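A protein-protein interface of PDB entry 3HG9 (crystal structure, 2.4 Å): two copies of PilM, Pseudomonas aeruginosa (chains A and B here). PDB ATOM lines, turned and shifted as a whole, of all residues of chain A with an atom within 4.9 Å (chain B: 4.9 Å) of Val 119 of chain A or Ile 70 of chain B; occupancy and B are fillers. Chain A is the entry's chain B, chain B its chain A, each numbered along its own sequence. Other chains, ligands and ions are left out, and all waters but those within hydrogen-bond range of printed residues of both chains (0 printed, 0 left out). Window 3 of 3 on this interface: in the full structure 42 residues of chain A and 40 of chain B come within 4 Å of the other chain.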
ATOM      1  N   GLY A  91     -21.256 -21.675 -15.884  1.00  0.00           N
ATOM      2  CA  GLY A  91     -20.540 -22.650 -16.691  1.00  0.00           C
ATOM      3  C   GLY A  91     -19.046 -22.537 -16.389  1.00  0.00           C
ATOM      4  O   GLY A  91     -18.616 -21.646 -15.645  1.00  0.00           O
ATOM      5  N   VAL A  92     -18.261 -23.444 -16.978  1.00  0.00           N
ATOM      6  CA  VAL A  92     -16.840 -23.624 -16.665  1.00  0.00           C
ATOM      7  C   VAL A  92     -16.071 -22.778 -17.638  1.00  0.00           C
ATOM      8  O   VAL A  92     -16.507 -22.666 -18.795  1.00  0.00           O
ATOM      9  CB  VAL A  92     -16.448 -25.083 -16.903  1.00  0.00           C
ATOM     10  CG1 VAL A  92     -14.865 -25.286 -16.946  1.00  0.00           C
ATOM     11  CG2 VAL A  92     -17.171 -25.985 -15.898  1.00  0.00           C
ATOM     12  N   GLY A 117     -10.494 -23.071 -16.074  1.00  0.00           N
ATOM     13  CA  GLY A 117     -11.290 -24.151 -15.514  1.00  0.00           C
ATOM     14  C   GLY A 117     -12.147 -23.782 -14.307  1.00  0.00           C
ATOM     15  O   GLY A 117     -12.738 -24.665 -13.681  1.00  0.00           O
ATOM     16  N   ALA A 118     -12.239 -22.512 -13.947  1.00  0.00           N
ATOM     17  CA  ALA A 118     -13.029 -22.182 -12.740  1.00  0.00           C
ATOM     18  C   ALA A 118     -14.508 -22.329 -13.066  1.00  0.00           C
ATOM     19  O   ALA A 118     -14.918 -21.913 -14.160  1.00  0.00           O
ATOM     20  CB  ALA A 118     -12.732 -20.767 -12.238  1.00  0.00           C
ATOM     21  N   VAL A 119     -15.307 -22.916 -12.157  1.00  0.00           N
ATOM     22  CA  VAL A 119     -16.782 -22.839 -12.308  1.00  0.00           C
ATOM     23  C   VAL A 119     -17.274 -21.472 -11.839  1.00  0.00           C
ATOM     24  O   VAL A 119     -16.783 -20.947 -10.825  1.00  0.00           O
ATOM     25  CB  VAL A 119     -17.562 -23.991 -11.581  1.00  0.00           C
ATOM     26  CG1 VAL A 119     -19.119 -23.860 -11.794  1.00  0.00           C
ATOM     27  CG2 VAL A 119     -17.100 -25.371 -12.093  1.00  0.00           C
ATOM     28  N   VAL A 120     -18.225 -20.916 -12.587  1.00  0.00           N
ATOM     29  CA  VAL A 120     -18.575 -19.488 -12.543  1.00  0.00           C
ATOM     30  C   VAL A 120     -20.096 -19.175 -12.596  1.00  0.00           C
ATOM     31  O   VAL A 120     -20.803 -19.545 -13.550  1.00  0.00           O
ATOM     32  CB  VAL A 120     -18.046 -18.730 -13.814  1.00  0.00           C
ATOM     33  CG1 VAL A 120     -17.785 -17.249 -13.495  1.00  0.00           C
ATOM     34  CG2 VAL A 120     -16.826 -19.374 -14.438  1.00  0.00           C
ATOM     35  N   ALA A 121     -20.593 -18.394 -11.659  1.00  0.00           N
ATOM     36  CA  ALA A 121     -21.951 -17.914 -11.785  1.00  0.00           C
ATOM     37  C   ALA A 121     -21.969 -16.452 -12.129  1.00  0.00           C
ATOM     38  O   ALA A 121     -21.345 -15.634 -11.412  1.00  0.00           O
ATOM     39  CB  ALA A 121     -22.707 -18.115 -10.479  1.00  0.00           C
ATOM     40  N   LEU B  15     -22.339 -26.733  -1.435  1.00  0.00           N
ATOM     41  CA  LEU B  15     -21.288 -25.850  -1.921  1.00  0.00           C
ATOM     42  C   LEU B  15     -21.801 -25.014  -3.079  1.00  0.00           C
ATOM     43  O   LEU B  15     -21.373 -23.871  -3.272  1.00  0.00           O
ATOM     44  CB  LEU B  15     -20.015 -26.598  -2.319  1.00  0.00           C
ATOM     45  CG  LEU B  15     -18.883 -25.672  -2.838  1.00  0.00           C
ATOM     46  CD1 LEU B  15     -18.418 -24.591  -1.810  1.00  0.00           C
ATOM     47  CD2 LEU B  15     -17.647 -26.469  -3.418  1.00  0.00           C
ATOM     48  N   LEU B  19     -22.034 -20.724  -3.204  1.00  0.00           N
ATOM     49  CA  LEU B  19     -21.659 -19.915  -4.329  1.00  0.00           C
ATOM     50  C   LEU B  19     -22.814 -19.001  -4.795  1.00  0.00           C
ATOM     51  O   LEU B  19     -22.570 -17.823  -5.039  1.00  0.00           O
ATOM     52  CB  LEU B  19     -21.220 -20.853  -5.439  1.00  0.00           C
ATOM     53  CG  LEU B  19     -20.478 -20.226  -6.575  1.00  0.00           C
ATOM     54  CD1 LEU B  19     -19.708 -21.375  -7.196  1.00  0.00           C
ATOM     55  CD2 LEU B  19     -21.358 -19.591  -7.597  1.00  0.00           C
ATOM     56  N   ARG B  56     -11.558 -19.738  -1.637  1.00  0.00           N
ATOM     57  CA  ARG B  56     -11.621 -20.572  -2.868  1.00  0.00           C
ATOM     58  C   ARG B  56     -12.946 -20.253  -3.603  1.00  0.00           C
ATOM     59  O   ARG B  56     -13.084 -20.453  -4.827  1.00  0.00           O
ATOM     60  CB  ARG B  56     -11.421 -22.105  -2.690  1.00  0.00           C
ATOM     61  CG  ARG B  56     -12.310 -22.972  -1.655  1.00  0.00           C
ATOM     62  CD  ARG B  56     -11.341 -24.076  -1.075  1.00  0.00           C
ATOM     63  NE  ARG B  56     -11.355 -24.472   0.356  1.00  0.00           N
ATOM     64  CZ  ARG B  56     -10.923 -23.818   1.434  1.00  0.00           C
ATOM     65  NH1 ARG B  56     -10.498 -22.595   1.430  1.00  0.00           N
ATOM     66  NH2 ARG B  56     -11.048 -24.407   2.571  1.00  0.00           N
ATOM     67  N   LEU B  57     -13.874 -19.701  -2.839  1.00  0.00           N
ATOM     68  CA  LEU B  57     -15.065 -19.086  -3.351  1.00  0.00           C
ATOM     69  C   LEU B  57     -14.831 -17.588  -3.490  1.00  0.00           C
ATOM     70  O   LEU B  57     -14.926 -16.825  -2.506  1.00  0.00           O
ATOM     71  CB  LEU B  57     -16.206 -19.345  -2.333  1.00  0.00           C
ATOM     72  CG  LEU B  57     -17.555 -19.668  -2.877  1.00  0.00           C
ATOM     73  CD1 LEU B  57     -18.547 -19.997  -1.685  1.00  0.00           C
ATOM     74  CD2 LEU B  57     -17.946 -18.501  -3.822  1.00  0.00           C
ATOM     75  N   ALA B  68     -19.158 -15.107  -9.618  1.00  0.00           N
ATOM     76  CA  ALA B  68     -18.751 -15.816  -8.413  1.00  0.00           C
ATOM     77  C   ALA B  68     -18.106 -17.127  -8.879  1.00  0.00           C
ATOM     78  O   ALA B  68     -18.681 -17.810  -9.774  1.00  0.00           O
ATOM     79  CB  ALA B  68     -19.992 -16.067  -7.480  1.00  0.00           C
ATOM     80  N   PHE B  69     -16.932 -17.469  -8.336  1.00  0.00           N
ATOM     81  CA  PHE B  69     -16.235 -18.602  -8.872  1.00  0.00           C
ATOM     82  C   PHE B  69     -15.467 -19.445  -7.931  1.00  0.00           C
ATOM     83  O   PHE B  69     -15.124 -19.020  -6.833  1.00  0.00           O
ATOM     84  CB  PHE B  69     -15.298 -18.186 -10.005  1.00  0.00           C
ATOM     85  CG  PHE B  69     -14.335 -17.115  -9.643  1.00  0.00           C
ATOM     86  CD1 PHE B  69     -13.026 -17.413  -9.391  1.00  0.00           C
ATOM     87  CD2 PHE B  69     -14.753 -15.804  -9.556  1.00  0.00           C
ATOM     88  CE1 PHE B  69     -12.149 -16.453  -9.094  1.00  0.00           C
ATOM     89  CE2 PHE B  69     -13.875 -14.816  -9.219  1.00  0.00           C
ATOM     90  CZ  PHE B  69     -12.552 -15.127  -9.010  1.00  0.00           C
ATOM     91  N   ILE B  70     -15.216 -20.657  -8.407  1.00  0.00           N
ATOM     92  CA  ILE B  70     -14.393 -21.620  -7.722  1.00  0.00           C
ATOM     93  C   ILE B  70     -13.350 -22.183  -8.682  1.00  0.00           C
ATOM     94  O   ILE B  70     -13.647 -22.999  -9.525  1.00  0.00           O
ATOM     95  CB  ILE B  70     -15.240 -22.758  -7.104  1.00  0.00           C
ATOM     96  CG1 ILE B  70     -16.245 -22.130  -6.145  1.00  0.00           C
ATOM     97  CG2 ILE B  70     -14.330 -23.806  -6.393  1.00  0.00           C
ATOM     98  CD1 ILE B  70     -16.771 -23.047  -5.023  1.00  0.00           C
ATOM     99  N   ALA B  71     -12.121 -21.753  -8.484  1.00  0.00           N
ATOM    100  CA  ALA B  71     -10.979 -22.059  -9.347  1.00  0.00           C
ATOM    101  C   ALA B  71     -10.477 -23.536  -9.470  1.00  0.00           C
ATOM    102  O   ALA B  71      -9.973 -23.941 -10.521  1.00  0.00           O
ATOM    103  CB  ALA B  71      -9.799 -21.084  -9.021  1.00  0.00           C
ATOM    104  N   SER B  72     -10.603 -24.351  -8.439  1.00  0.00           N
ATOM    105  CA  SER B  72     -10.100 -25.725  -8.593  1.00  0.00           C
ATOM    106  C   SER B  72     -11.242 -26.635  -8.316  1.00  0.00           C
ATOM    107  O   SER B  72     -11.164 -27.485  -7.442  1.00  0.00           O
ATOM    108  CB  SER B  72      -8.945 -26.002  -7.608  1.00  0.00           C
ATOM    109  OG  SER B  72      -8.525 -27.360  -7.697  1.00  0.00           O
ATOM    110  N   PRO B  73     -12.310 -26.483  -9.093  1.00  0.00           N
ATOM    111  CA  PRO B  73     -13.604 -26.859  -8.551  1.00  0.00           C
ATOM    112  C   PRO B  73     -13.809 -28.382  -8.542  1.00  0.00           C
ATOM    113  O   PRO B  73     -13.516 -29.041  -9.531  1.00  0.00           O
ATOM    114  CB  PRO B  73     -14.567 -26.118  -9.477  1.00  0.00           C
ATOM    115  CG  PRO B  73     -13.811 -25.992 -10.822  1.00  0.00           C
ATOM    116  CD  PRO B  73     -12.353 -26.220 -10.555  1.00  0.00           C
ATOM    117  N   PRO B  74     -14.247 -28.944  -7.397  1.00  0.00           N
ATOM    118  CA  PRO B  74     -14.605 -30.344  -7.249  1.00  0.00           C
ATOM    119  C   PRO B  74     -15.522 -30.785  -8.339  1.00  0.00           C
ATOM    120  O   PRO B  74     -16.484 -30.079  -8.645  1.00  0.00           O
ATOM    121  CB  PRO B  74     -15.390 -30.346  -5.941  1.00  0.00           C
ATOM    122  CG  PRO B  74     -14.649 -29.381  -5.120  1.00  0.00           C
ATOM    123  CD  PRO B  74     -14.289 -28.257  -6.084  1.00  0.00           C
ATOM    124  N   LEU B  77     -19.665 -30.074  -9.091  1.00  0.00           N
ATOM    125  CA  LEU B  77     -20.068 -28.689  -8.803  1.00  0.00           C
ATOM    126  C   LEU B  77     -20.664 -27.954 -10.014  1.00  0.00           C
ATOM    127  O   LEU B  77     -21.698 -27.252  -9.859  1.00  0.00           O
ATOM    128  CB  LEU B  77     -18.883 -27.904  -8.249  1.00  0.00           C
ATOM    129  CG  LEU B  77     -19.110 -26.465  -7.812  1.00  0.00           C
ATOM    130  CD1 LEU B  77     -19.852 -26.348  -6.520  1.00  0.00           C
ATOM    131  CD2 LEU B  77     -17.739 -25.846  -7.690  1.00  0.00           C
ATOM    132  N   ALA B  78     -20.036 -28.116 -11.198  1.00  0.00           N
ATOM    133  CA  ALA B  78     -20.576 -27.566 -12.489  1.00  0.00           C
ATOM    134  C   ALA B  78     -22.030 -27.851 -12.614  1.00  0.00           C
ATOM    135  O   ALA B  78     -22.820 -26.933 -12.847  1.00  0.00           O
ATOM    136  CB  ALA B  78     -19.861 -28.139 -13.690  1.00  0.00           C
ATOM    137  N   VAL B  81     -24.276 -26.426  -9.704  1.00  0.00           N
ATOM    138  CA  VAL B  81     -24.579 -24.998  -9.769  1.00  0.00           C
ATOM    139  C   VAL B  81     -25.575 -24.679 -10.863  1.00  0.00           C
ATOM    140  O   VAL B  81     -26.460 -23.812 -10.724  1.00  0.00           O
ATOM    141  CB  VAL B  81     -23.342 -24.147  -9.920  1.00  0.00           C
ATOM    142  CG1 VAL B  81     -23.723 -22.689  -9.732  1.00  0.00           C
ATOM    143  CG2 VAL B  81     -22.278 -24.566  -8.865  1.00  0.00           C
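The backbone NH (N) of Ile 70 of chain B is in hydrogen-bond range of the backbone carbonyl oxygen (O) of Val 119 of chain A, 2.9 Å away. The backbone NH (N) of Ala 121 of chain A is in hydrogen-bond range of the backbone carbonyl oxygen (O) of Ala 68 of chain B (2.7 Å).
The backbone carbonyl oxygen (O) of Gly 91 of chain A sits close to the backbone NH (N) of Val 120 of chain A, at 3.2 Å.
Gly 117 of chain A touches Pro 73 of chain B. Ala 118 of chain A touches Ile 70 of chain B. CB of Ala 118 of chain A touches CA of Ala 71 of chain B, at 3.6 Å. O of Val 119 of chain A touches O of Ala 68 of chain B, 3.8 Å away. O of Val 119 of chain A touches CA of Phe 69 of chain B, 3.1 Å away. Val 119 of chain A touches Pro 73 of chain B. Val 120 of chain A touches Ala 68 of chain B. Ala 121 of chain A touches Leu 19 of chain B.
Val 119 of chain A touches four residues of chain B. Printed residues of chain A within 4 Å of Phe 69 of chain B: Val 119. Of the printed residues of chain A, Ala 71 of chain B touches Ala 118 (3.6 Å). Pro 74 of chain B touches none of the printed residues of chain A. Leu 57 of chain B touches none of the printed residues of chain A. The nearest residue of chain B that does not touch Val 119 of chain A is Ala 78 of chain B (4.04 Å). The nearest printed residue of chain B that does not touch Ala 121 of chain A is Val 81 of chain B (4.7 Å).
Hydrophobic or aromatic side chains of chain B that line the printed part of chain A: Leu 19, Phe 69 and Pro 73. Of the 7 printed residues of chain A, 5 touch a printed residue of chain B. Printed residues of chain A that touch a printed residue of chain B: Gly 117, Ala 118, Val 119, Val 120 and Ala 121. Hydrophobic or aromatic side chains of chain A that line the printed part of chain B: Ala 118, Val 119, Val 120 and Ala 121. Among the printed residues, 10 pairs touch across the chains.
No position is printed for both chains.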
